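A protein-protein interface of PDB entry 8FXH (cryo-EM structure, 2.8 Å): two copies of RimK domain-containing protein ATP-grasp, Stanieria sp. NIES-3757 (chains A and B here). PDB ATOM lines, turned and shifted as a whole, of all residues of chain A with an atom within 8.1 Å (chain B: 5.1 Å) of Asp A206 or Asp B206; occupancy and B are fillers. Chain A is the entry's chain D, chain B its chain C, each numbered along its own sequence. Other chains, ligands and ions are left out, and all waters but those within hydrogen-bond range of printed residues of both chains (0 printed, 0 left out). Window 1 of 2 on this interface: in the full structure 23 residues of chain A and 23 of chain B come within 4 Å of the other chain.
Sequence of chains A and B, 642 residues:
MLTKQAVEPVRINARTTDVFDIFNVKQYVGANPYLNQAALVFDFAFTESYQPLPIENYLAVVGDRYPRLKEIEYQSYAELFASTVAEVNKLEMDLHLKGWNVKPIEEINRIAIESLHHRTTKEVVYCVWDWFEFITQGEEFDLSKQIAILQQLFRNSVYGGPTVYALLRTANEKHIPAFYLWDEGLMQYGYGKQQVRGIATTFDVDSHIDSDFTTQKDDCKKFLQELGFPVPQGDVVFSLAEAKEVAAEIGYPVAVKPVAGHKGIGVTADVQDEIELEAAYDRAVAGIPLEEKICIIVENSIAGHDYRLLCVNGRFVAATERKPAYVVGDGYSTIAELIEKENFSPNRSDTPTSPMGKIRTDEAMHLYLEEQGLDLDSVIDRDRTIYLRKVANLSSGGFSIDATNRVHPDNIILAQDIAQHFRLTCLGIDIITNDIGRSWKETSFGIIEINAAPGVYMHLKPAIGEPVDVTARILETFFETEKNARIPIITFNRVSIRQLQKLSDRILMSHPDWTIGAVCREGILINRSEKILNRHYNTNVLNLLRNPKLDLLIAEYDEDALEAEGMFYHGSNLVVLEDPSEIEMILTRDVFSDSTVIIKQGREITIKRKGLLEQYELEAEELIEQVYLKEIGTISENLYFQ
The backbone NH (N) of His A208 is in hydrogen-bond range of the backbone carbonyl oxygen (O) of Asp B206 (3.4 Å).
O of Asp A206 sits at hydrogen-bond distance from N of His B208 (3.4 Å).
OG of Ser B207 sits at hydrogen-bond distance from O of Asp A204 (2.7 Å).
The backbone carbonyl oxygen of Asp B204 sits at hydrogen-bond distance from the side-chain hydroxyl of Ser A207 (2.7 Å).
ND1 of His A208 is in hydrogen-bond range of ND1 of His B208, at 3.3 Å.
The side-chain carboxylate (OD2) of Asp A210 sits at hydrogen-bond distance from the backbone NH (N) of Arg A423, 2.6 Å away.
The backbone carbonyl oxygen (O) of Ser A207 lies within hydrogen-bond range of the side-chain hydroxyl (OG) of Ser A211 (3.1 Å).
N of Ser B207 is in hydrogen-bond range of O of Arg B423.
The guanidinium group (NH2) of Arg A197 is in salt-bridge range of the side-chain carboxylate (OD2) of Asp A204.
OD1 of Asp B206 is in hydrogen-bond range of OG1 of Thr B425 (3.1 Å).
The backbone carbonyl oxygen (O) of Arg A423 is in hydrogen-bond range of the backbone NH (N) of Ser A207 (3.4 Å).
Arg B423 touches Asp A204.
Asp A206 touches Asp B206.
Asp A206 touches Ser B207.
Asp B206 touches Ser A207 (O to CA, 3.7 Å).
Ser A207 touches His B208.
His A208 touches Ser B207.
Asp B204 touches Arg A423 (O to NE, 3.9 Å).
Asp A206 touches just these residues of chain B: Asp B206 (3.7 Å), Ser B207 (3.7 Å) and His B208 (3.4 Å).
Asp B206 touches just these residues of chain A: Asp A206, Ser A207 and His A208.
Printed residues of chain B within 4 Å of His A208: Asp B206, Ser B207 and His B208.
Printed residues of chain B within 4 Å of Asp A204: Ser B207 and Arg B423.
Ile A199 touches none of the printed residues of chain B.
Pro A454 touches none of the printed residues of chain B.
Printed residues of chain B that touch a printed residue of chain A: Asp B204, Asp B206, Ser B207, His B208 and Arg B423.
Hydrophobic or aromatic side chains of chain B within 4 Å of the printed part of chain A: His B208.
Among the printed residues, no Asp or Glu carboxylate lies within 4 Å of a Lys or Arg side-chain nitrogen of the other chain.
Asp A204 touches Ser B207, and with the chains exchanged Ser A207 touches Asp B204.
Asp A204 touches Arg B423, and with the chains exchanged Arg A423 touches Asp B204.
Asp A206 touches His B208, and with the chains exchanged His A208 touches Asp B206.
His A208 touches its own counterpart, His B208.
Positions printed for both chains: 201, 202, 203, 204, 205, 206, 207, 208, 423, 424 and 425.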
ATOM      1  N   ARG A 197     -12.853 -33.770 -21.093  1.00  0.00           N
ATOM      2  CA  ARG A 197     -13.019 -33.523 -19.668  1.00  0.00           C
ATOM      3  C   ARG A 197     -12.424 -32.171 -19.309  1.00  0.00           C
ATOM      4  O   ARG A 197     -11.390 -31.780 -19.850  1.00  0.00           O
ATOM      5  CB  ARG A 197     -12.348 -34.614 -18.837  1.00  0.00           C
ATOM      6  CG  ARG A 197     -12.828 -36.010 -19.146  1.00  0.00           C
ATOM      7  CD  ARG A 197     -12.043 -37.035 -18.367  1.00  0.00           C
ATOM      8  NE  ARG A 197     -10.759 -37.321 -18.994  1.00  0.00           N
ATOM      9  CZ  ARG A 197      -9.587 -37.173 -18.396  1.00  0.00           C
ATOM     10  NH1 ARG A 197      -9.496 -36.743 -17.150  1.00  0.00           N
ATOM     11  NH2 ARG A 197      -8.477 -37.468 -19.064  1.00  0.00           N
ATOM     12  N   ILE A 199     -12.546 -28.486 -16.330  1.00  0.00           N
ATOM     13  CA  ILE A 199     -13.001 -27.718 -15.176  1.00  0.00           C
ATOM     14  C   ILE A 199     -12.930 -26.245 -15.558  1.00  0.00           C
ATOM     15  O   ILE A 199     -11.840 -25.720 -15.817  1.00  0.00           O
ATOM     16  CB  ILE A 199     -12.172 -28.003 -13.914  1.00  0.00           C
ATOM     17  CG1 ILE A 199     -12.445 -26.951 -12.841  1.00  0.00           C
ATOM     18  CG2 ILE A 199     -10.692 -28.089 -14.235  1.00  0.00           C
ATOM     19  CD1 ILE A 199     -13.819 -27.042 -12.237  1.00  0.00           C
ATOM     20  N   THR A 201     -12.495 -23.267 -17.522  1.00  0.00           N
ATOM     21  CA  THR A 201     -11.857 -22.997 -18.804  1.00  0.00           C
ATOM     22  C   THR A 201     -10.758 -24.000 -19.137  1.00  0.00           C
ATOM     23  O   THR A 201     -10.555 -24.317 -20.313  1.00  0.00           O
ATOM     24  CB  THR A 201     -11.289 -21.575 -18.811  1.00  0.00           C
ATOM     25  OG1 THR A 201     -12.366 -20.634 -18.813  1.00  0.00           O
ATOM     26  CG2 THR A 201     -10.445 -21.333 -20.040  1.00  0.00           C
ATOM     27  N   THR A 202     -10.057 -24.522 -18.135  1.00  0.00           N
ATOM     28  CA  THR A 202      -9.006 -25.496 -18.381  1.00  0.00           C
ATOM     29  C   THR A 202      -9.586 -26.805 -18.900  1.00  0.00           C
ATOM     30  O   THR A 202     -10.607 -27.287 -18.407  1.00  0.00           O
ATOM     31  CB  THR A 202      -8.220 -25.756 -17.099  1.00  0.00           C
ATOM     32  OG1 THR A 202      -8.042 -24.526 -16.391  1.00  0.00           O
ATOM     33  CG2 THR A 202      -6.861 -26.343 -17.418  1.00  0.00           C
ATOM     34  N   PHE A 203      -8.923 -27.387 -19.896  1.00  0.00           N
ATOM     35  CA  PHE A 203      -9.330 -28.659 -20.475  1.00  0.00           C
ATOM     36  C   PHE A 203      -8.177 -29.649 -20.393  1.00  0.00           C
ATOM     37  O   PHE A 203      -7.053 -29.300 -20.033  1.00  0.00           O
ATOM     38  CB  PHE A 203      -9.794 -28.491 -21.925  1.00  0.00           C
ATOM     39  CG  PHE A 203     -11.067 -27.714 -22.063  1.00  0.00           C
ATOM     40  CD1 PHE A 203     -12.282 -28.298 -21.765  1.00  0.00           C
ATOM     41  CD2 PHE A 203     -11.049 -26.402 -22.484  1.00  0.00           C
ATOM     42  CE1 PHE A 203     -13.453 -27.586 -21.885  1.00  0.00           C
ATOM     43  CE2 PHE A 203     -12.217 -25.686 -22.605  1.00  0.00           C
ATOM     44  CZ  PHE A 203     -13.419 -26.279 -22.305  1.00  0.00           C
ATOM     45  N   ASP A 204      -8.470 -30.902 -20.731  1.00  0.00           N
ATOM     46  CA  ASP A 204      -7.503 -31.982 -20.580  1.00  0.00           C
ATOM     47  C   ASP A 204      -6.455 -32.027 -21.684  1.00  0.00           C
ATOM     48  O   ASP A 204      -5.510 -32.814 -21.582  1.00  0.00           O
ATOM     49  CB  ASP A 204      -8.235 -33.328 -20.469  1.00  0.00           C
ATOM     50  CG  ASP A 204      -8.723 -33.869 -21.813  1.00  0.00           C
ATOM     51  OD1 ASP A 204      -8.602 -33.191 -22.852  1.00  0.00           O
ATOM     52  OD2 ASP A 204      -9.297 -34.978 -21.820  1.00  0.00           O
ATOM     53  N   VAL A 205      -6.596 -31.219 -22.735  1.00  0.00           N
ATOM     54  CA  VAL A 205      -5.618 -31.200 -23.816  1.00  0.00           C
ATOM     55  C   VAL A 205      -4.535 -30.149 -23.613  1.00  0.00           C
ATOM     56  O   VAL A 205      -3.594 -30.087 -24.419  1.00  0.00           O
ATOM     57  CB  VAL A 205      -6.300 -30.980 -25.183  1.00  0.00           C
ATOM     58  CG1 VAL A 205      -7.054 -32.220 -25.595  1.00  0.00           C
ATOM     59  CG2 VAL A 205      -7.229 -29.793 -25.117  1.00  0.00           C
ATOM     60  N   ASP A 206      -4.635 -29.325 -22.577  1.00  0.00           N
ATOM     61  CA  ASP A 206      -3.628 -28.311 -22.316  1.00  0.00           C
ATOM     62  C   ASP A 206      -2.361 -28.944 -21.758  1.00  0.00           C
ATOM     63  O   ASP A 206      -2.397 -29.998 -21.120  1.00  0.00           O
ATOM     64  CB  ASP A 206      -4.161 -27.266 -21.342  1.00  0.00           C
ATOM     65  CG  ASP A 206      -5.392 -26.564 -21.866  1.00  0.00           C
ATOM     66  OD1 ASP A 206      -5.854 -26.924 -22.965  1.00  0.00           O
ATOM     67  OD2 ASP A 206      -5.896 -25.649 -21.183  1.00  0.00           O
ATOM     68  N   SER A 207      -1.235 -28.283 -21.999  1.00  0.00           N
ATOM     69  CA  SER A 207       0.071 -28.824 -21.656  1.00  0.00           C
ATOM     70  C   SER A 207       0.451 -28.479 -20.224  1.00  0.00           C
ATOM     71  O   SER A 207       0.091 -27.420 -19.710  1.00  0.00           O
ATOM     72  CB  SER A 207       1.132 -28.292 -22.614  1.00  0.00           C
ATOM     73  OG  SER A 207       2.351 -28.989 -22.455  1.00  0.00           O
ATOM     74  N   HIS A 208       1.186 -29.389 -19.585  1.00  0.00           N
ATOM     75  CA  HIS A 208       1.648 -29.171 -18.220  1.00  0.00           C
ATOM     76  C   HIS A 208       2.824 -28.209 -18.163  1.00  0.00           C
ATOM     77  O   HIS A 208       3.029 -27.547 -17.141  1.00  0.00           O
ATOM     78  CB  HIS A 208       2.029 -30.508 -17.585  1.00  0.00           C
ATOM     79  CG  HIS A 208       2.552 -30.393 -16.189  1.00  0.00           C
ATOM     80  ND1 HIS A 208       1.770 -29.981 -15.132  1.00  0.00           N
ATOM     81  CD2 HIS A 208       3.774 -30.656 -15.671  1.00  0.00           C
ATOM     82  CE1 HIS A 208       2.491 -29.985 -14.026  1.00  0.00           C
ATOM     83  NE2 HIS A 208       3.711 -30.390 -14.325  1.00  0.00           N
ATOM     84  N   ILE A 209       3.603 -28.122 -19.238  1.00  0.00           N
ATOM     85  CA  ILE A 209       4.797 -27.285 -19.239  1.00  0.00           C
ATOM     86  C   ILE A 209       4.446 -25.828 -19.503  1.00  0.00           C
ATOM     87  O   ILE A 209       5.001 -24.920 -18.873  1.00  0.00           O
ATOM     88  CB  ILE A 209       5.797 -27.826 -20.272  1.00  0.00           C
ATOM     89  CG1 ILE A 209       6.525 -29.048 -19.716  1.00  0.00           C
ATOM     90  CG2 ILE A 209       6.782 -26.757 -20.674  1.00  0.00           C
ATOM     91  CD1 ILE A 209       7.372 -29.755 -20.732  1.00  0.00           C
ATOM     92  N   ASP A 210       3.527 -25.580 -20.436  1.00  0.00           N
ATOM     93  CA  ASP A 210       3.215 -24.212 -20.833  1.00  0.00           C
ATOM     94  C   ASP A 210       2.558 -23.428 -19.705  1.00  0.00           C
ATOM     95  O   ASP A 210       2.830 -22.235 -19.536  1.00  0.00           O
ATOM     96  CB  ASP A 210       2.322 -24.224 -22.069  1.00  0.00           C
ATOM     97  CG  ASP A 210       3.062 -24.667 -23.310  1.00  0.00           C
ATOM     98  OD1 ASP A 210       4.194 -25.170 -23.175  1.00  0.00           O
ATOM     99  OD2 ASP A 210       2.518 -24.512 -24.422  1.00  0.00           O
ATOM    100  N   SER A 211       1.682 -24.070 -18.932  1.00  0.00           N
ATOM    101  CA  SER A 211       1.045 -23.380 -17.815  1.00  0.00           C
ATOM    102  C   SER A 211       2.074 -22.955 -16.776  1.00  0.00           C
ATOM    103  O   SER A 211       2.043 -21.824 -16.274  1.00  0.00           O
ATOM    104  CB  SER A 211      -0.015 -24.277 -17.187  1.00  0.00           C
ATOM    105  OG  SER A 211      -0.838 -24.850 -18.184  1.00  0.00           O
ATOM    106  N   ARG A 423       0.728 -24.254 -26.336  1.00  0.00           N
ATOM    107  CA  ARG A 423      -0.226 -25.353 -26.481  1.00  0.00           C
ATOM    108  C   ARG A 423      -1.350 -25.230 -25.454  1.00  0.00           C
ATOM    109  O   ARG A 423      -1.521 -26.065 -24.572  1.00  0.00           O
ATOM    110  CB  ARG A 423       0.490 -26.694 -26.355  1.00  0.00           C
ATOM    111  CG  ARG A 423       1.195 -27.140 -27.614  1.00  0.00           C
ATOM    112  CD  ARG A 423       1.812 -28.510 -27.438  1.00  0.00           C
ATOM    113  NE  ARG A 423       0.814 -29.571 -27.466  1.00  0.00           N
ATOM    114  CZ  ARG A 423       0.634 -30.399 -28.485  1.00  0.00           C
ATOM    115  NH1 ARG A 423       1.367 -30.316 -29.581  1.00  0.00           N
ATOM    116  NH2 ARG A 423      -0.304 -31.336 -28.401  1.00  0.00           N
ATOM    117  N   LEU A 424      -2.123 -24.157 -25.585  1.00  0.00           N
ATOM    118  CA  LEU A 424      -3.263 -23.899 -24.721  1.00  0.00           C
ATOM    119  C   LEU A 424      -4.466 -23.540 -25.577  1.00  0.00           C
ATOM    120  O   LEU A 424      -4.322 -23.042 -26.695  1.00  0.00           O
ATOM    121  CB  LEU A 424      -2.978 -22.774 -23.727  1.00  0.00           C
ATOM    122  CG  LEU A 424      -1.708 -22.908 -22.892  1.00  0.00           C
ATOM    123  CD1 LEU A 424      -1.371 -21.596 -22.221  1.00  0.00           C
ATOM    124  CD2 LEU A 424      -1.863 -24.001 -21.866  1.00  0.00           C
ATOM    125  N   THR A 425      -5.657 -23.799 -25.043  1.00  0.00           N
ATOM    126  CA  THR A 425      -6.874 -23.537 -25.803  1.00  0.00           C
ATOM    127  C   THR A 425      -7.273 -22.067 -25.744  1.00  0.00           C
ATOM    128  O   THR A 425      -7.575 -21.467 -26.778  1.00  0.00           O
ATOM    129  CB  THR A 425      -8.013 -24.412 -25.290  1.00  0.00           C
ATOM    130  OG1 THR A 425      -7.579 -25.776 -25.238  1.00  0.00           O
ATOM    131  CG2 THR A 425      -9.214 -24.309 -26.207  1.00  0.00           C
ATOM    132  N   CYS A 426      -7.277 -21.476 -24.554  1.00  0.00           N
ATOM    133  CA  CYS A 426      -7.652 -20.082 -24.369  1.00  0.00           C
ATOM    134  C   CYS A 426      -6.497 -19.323 -23.735  1.00  0.00           C
ATOM    135  O   CYS A 426      -5.837 -19.829 -22.824  1.00  0.00           O
ATOM    136  CB  CYS A 426      -8.895 -19.956 -23.490  1.00  0.00           C
ATOM    137  SG  CYS A 426     -10.250 -21.043 -23.958  1.00  0.00           S
ATOM    138  N   ALA A 452      -3.180 -17.998 -18.594  1.00  0.00           N
ATOM    139  CA  ALA A 452      -3.488 -19.270 -19.235  1.00  0.00           C
ATOM    140  C   ALA A 452      -4.918 -19.735 -19.008  1.00  0.00           C
ATOM    141  O   ALA A 452      -5.464 -20.455 -19.851  1.00  0.00           O
ATOM    142  CB  ALA A 452      -2.527 -20.353 -18.738  1.00  0.00           C
ATOM    143  N   ALA A 453      -5.541 -19.352 -17.898  1.00  0.00           N
ATOM    144  CA  ALA A 453      -6.911 -19.754 -17.580  1.00  0.00           C
ATOM    145  C   ALA A 453      -7.721 -18.499 -17.292  1.00  0.00           C
ATOM    146  O   ALA A 453      -8.033 -18.195 -16.133  1.00  0.00           O
ATOM    147  CB  ALA A 453      -6.950 -20.721 -16.399  1.00  0.00           C
ATOM    148  N   PRO A 454      -8.079 -17.744 -18.325  1.00  0.00           N
ATOM    149  CA  PRO A 454      -8.767 -16.473 -18.105  1.00  0.00           C
ATOM    150  C   PRO A 454     -10.238 -16.672 -17.783  1.00  0.00           C
ATOM    151  O   PRO A 454     -10.834 -17.714 -18.061  1.00  0.00           O
ATOM    152  CB  PRO A 454      -8.590 -15.753 -19.441  1.00  0.00           C
ATOM    153  CG  PRO A 454      -8.567 -16.859 -20.427  1.00  0.00           C
ATOM    154  CD  PRO A 454      -7.884 -18.020 -19.757  1.00  0.00           C
ATOM    155  N   PHE A 478     -13.940 -28.415 -30.543  1.00  0.00           N
ATOM    156  CA  PHE A 478     -13.897 -29.861 -30.390  1.00  0.00           C
ATOM    157  C   PHE A 478     -14.965 -30.576 -31.208  1.00  0.00           C
ATOM    158  O   PHE A 478     -14.642 -31.467 -31.996  1.00  0.00           O
ATOM    159  CB  PHE A 478     -14.041 -30.228 -28.911  1.00  0.00           C
ATOM    160  CG  PHE A 478     -13.078 -29.515 -28.016  1.00  0.00           C
ATOM    161  CD1 PHE A 478     -11.730 -29.807 -28.054  1.00  0.00           C
ATOM    162  CD2 PHE A 478     -13.520 -28.552 -27.130  1.00  0.00           C
ATOM    163  CE1 PHE A 478     -10.845 -29.154 -27.231  1.00  0.00           C
ATOM    164  CE2 PHE A 478     -12.638 -27.897 -26.307  1.00  0.00           C
ATOM    165  CZ  PHE A 478     -11.300 -28.199 -26.356  1.00  0.00           C
ATOM    166  N   THR B 201      11.950 -36.912 -18.507  1.00  0.00           N
ATOM    167  CA  THR B 201      10.888 -37.815 -18.935  1.00  0.00           C
ATOM    168  C   THR B 201       9.612 -37.080 -19.324  1.00  0.00           C
ATOM    169  O   THR B 201       8.897 -37.531 -20.224  1.00  0.00           O
ATOM    170  CB  THR B 201      10.594 -38.829 -17.826  1.00  0.00           C
ATOM    171  OG1 THR B 201      11.704 -39.721 -17.690  1.00  0.00           O
ATOM    172  CG2 THR B 201       9.366 -39.647 -18.152  1.00  0.00           C
ATOM    173  N   THR B 202       9.317 -35.952 -18.687  1.00  0.00           N
ATOM    174  CA  THR B 202       8.121 -35.191 -19.021  1.00  0.00           C
ATOM    175  C   THR B 202       8.229 -34.591 -20.416  1.00  0.00           C
ATOM    176  O   THR B 202       9.277 -34.071 -20.806  1.00  0.00           O
ATOM    177  CB  THR B 202       7.905 -34.078 -17.999  1.00  0.00           C
ATOM    178  OG1 THR B 202       8.225 -34.564 -16.692  1.00  0.00           O
ATOM    179  CG2 THR B 202       6.463 -33.616 -18.016  1.00  0.00           C
ATOM    180  N   PHE B 203       7.134 -34.656 -21.170  1.00  0.00           N
ATOM    181  CA  PHE B 203       7.067 -34.097 -22.510  1.00  0.00           C
ATOM    182  C   PHE B 203       5.914 -33.106 -22.593  1.00  0.00           C
ATOM    183  O   PHE B 203       5.106 -32.981 -21.672  1.00  0.00           O
ATOM    184  CB  PHE B 203       6.911 -35.192 -23.569  1.00  0.00           C
ATOM    185  CG  PHE B 203       8.116 -36.070 -23.707  1.00  0.00           C
ATOM    186  CD1 PHE B 203       9.241 -35.621 -24.368  1.00  0.00           C
ATOM    187  CD2 PHE B 203       8.127 -37.341 -23.169  1.00  0.00           C
ATOM    188  CE1 PHE B 203      10.352 -36.423 -24.491  1.00  0.00           C
ATOM    189  CE2 PHE B 203       9.237 -38.146 -23.290  1.00  0.00           C
ATOM    190  CZ  PHE B 203      10.348 -37.686 -23.951  1.00  0.00           C
ATOM    191  N   ASP B 204       5.846 -32.393 -23.713  1.00  0.00           N
ATOM    192  CA  ASP B 204       4.875 -31.319 -23.881  1.00  0.00           C
ATOM    193  C   ASP B 204       3.472 -31.808 -24.216  1.00  0.00           C
ATOM    194  O   ASP B 204       2.546 -30.993 -24.245  1.00  0.00           O
ATOM    195  CB  ASP B 204       5.372 -30.325 -24.940  1.00  0.00           C
ATOM    196  CG  ASP B 204       5.175 -30.812 -26.377  1.00  0.00           C
ATOM    197  OD1 ASP B 204       4.741 -31.958 -26.603  1.00  0.00           O
ATOM    198  OD2 ASP B 204       5.518 -30.049 -27.302  1.00  0.00           O
ATOM    199  N   VAL B 205       3.288 -33.101 -24.479  1.00  0.00           N
ATOM    200  CA  VAL B 205       1.966 -33.635 -24.788  1.00  0.00           C
ATOM    201  C   VAL B 205       1.239 -34.155 -23.556  1.00  0.00           C
ATOM    202  O   VAL B 205       0.070 -34.557 -23.669  1.00  0.00           O
ATOM    203  CB  VAL B 205       2.050 -34.752 -25.847  1.00  0.00           C
ATOM    204  CG1 VAL B 205       2.368 -34.166 -27.201  1.00  0.00           C
ATOM    205  CG2 VAL B 205       3.093 -35.771 -25.453  1.00  0.00           C
ATOM    206  N   ASP B 206       1.881 -34.165 -22.395  1.00  0.00           N
ATOM    207  CA  ASP B 206       1.240 -34.632 -21.178  1.00  0.00           C
ATOM    208  C   ASP B 206       0.235 -33.605 -20.674  1.00  0.00           C
ATOM    209  O   ASP B 206       0.369 -32.403 -20.912  1.00  0.00           O
ATOM    210  CB  ASP B 206       2.280 -34.918 -20.100  1.00  0.00           C
ATOM    211  CG  ASP B 206       3.276 -35.971 -20.524  1.00  0.00           C
ATOM    212  OD1 ASP B 206       3.183 -36.443 -21.673  1.00  0.00           O
ATOM    213  OD2 ASP B 206       4.150 -36.331 -19.710  1.00  0.00           O
ATOM    214  N   SER B 207      -0.776 -34.092 -19.962  1.00  0.00           N
ATOM    215  CA  SER B 207      -1.890 -33.265 -19.529  1.00  0.00           C
ATOM    216  C   SER B 207      -1.588 -32.587 -18.200  1.00  0.00           C
ATOM    217  O   SER B 207      -0.890 -33.141 -17.350  1.00  0.00           O
ATOM    218  CB  SER B 207      -3.157 -34.105 -19.403  1.00  0.00           C
ATOM    219  OG  SER B 207      -4.293 -33.283 -19.225  1.00  0.00           O
ATOM    220  N   HIS B 208      -2.122 -31.379 -18.032  1.00  0.00           N
ATOM    221  CA  HIS B 208      -1.942 -30.633 -16.792  1.00  0.00           C
ATOM    222  C   HIS B 208      -2.829 -31.159 -15.675  1.00  0.00           C
ATOM    223  O   HIS B 208      -2.490 -31.008 -14.497  1.00  0.00           O
ATOM    224  CB  HIS B 208      -2.227 -29.152 -17.037  1.00  0.00           C
ATOM    225  CG  HIS B 208      -2.103 -28.296 -15.815  1.00  0.00           C
ATOM    226  ND1 HIS B 208      -0.903 -28.081 -15.176  1.00  0.00           N
ATOM    227  CD2 HIS B 208      -3.027 -27.588 -15.127  1.00  0.00           C
ATOM    228  CE1 HIS B 208      -1.094 -27.284 -14.140  1.00  0.00           C
ATOM    229  NE2 HIS B 208      -2.376 -26.971 -14.087  1.00  0.00           N
ATOM    230  N   ARG B 423      -3.712 -39.580 -19.566  1.00  0.00           N
ATOM    231  CA  ARG B 423      -3.082 -38.968 -20.736  1.00  0.00           C
ATOM    232  C   ARG B 423      -1.630 -38.599 -20.435  1.00  0.00           C
ATOM    233  O   ARG B 423      -1.240 -37.437 -20.432  1.00  0.00           O
ATOM    234  CB  ARG B 423      -3.877 -37.747 -21.185  1.00  0.00           C
ATOM    235  CG  ARG B 423      -5.098 -38.074 -22.013  1.00  0.00           C
ATOM    236  CD  ARG B 423      -5.789 -36.813 -22.488  1.00  0.00           C
ATOM    237  NE  ARG B 423      -5.067 -36.165 -23.573  1.00  0.00           N
ATOM    238  CZ  ARG B 423      -5.450 -36.183 -24.841  1.00  0.00           C
ATOM    239  NH1 ARG B 423      -6.548 -36.814 -25.221  1.00  0.00           N
ATOM    240  NH2 ARG B 423      -4.716 -35.552 -25.751  1.00  0.00           N
ATOM    241  N   LEU B 424      -0.826 -39.626 -20.179  1.00  0.00           N
ATOM    242  CA  LEU B 424       0.594 -39.465 -19.911  1.00  0.00           C
ATOM    243  C   LEU B 424       1.376 -40.455 -20.758  1.00  0.00           C
ATOM    244  O   LEU B 424       0.863 -41.508 -21.140  1.00  0.00           O
ATOM    245  CB  LEU B 424       0.919 -39.676 -18.433  1.00  0.00           C
ATOM    246  CG  LEU B 424       0.102 -38.862 -17.433  1.00  0.00           C
ATOM    247  CD1 LEU B 424       0.276 -39.408 -16.034  1.00  0.00           C
ATOM    248  CD2 LEU B 424       0.498 -37.407 -17.486  1.00  0.00           C
ATOM    249  N   THR B 425       2.627 -40.106 -21.052  1.00  0.00           N
ATOM    250  CA  THR B 425       3.447 -40.964 -21.899  1.00  0.00           C
ATOM    251  C   THR B 425       4.053 -42.121 -21.117  1.00  0.00           C
ATOM    252  O   THR B 425       3.991 -43.270 -21.563  1.00  0.00           O
ATOM    253  CB  THR B 425       4.548 -40.145 -22.567  1.00  0.00           C
ATOM    254  OG1 THR B 425       3.971 -38.997 -23.196  1.00  0.00           O
ATOM    255  CG2 THR B 425       5.262 -40.976 -23.612  1.00  0.00           C
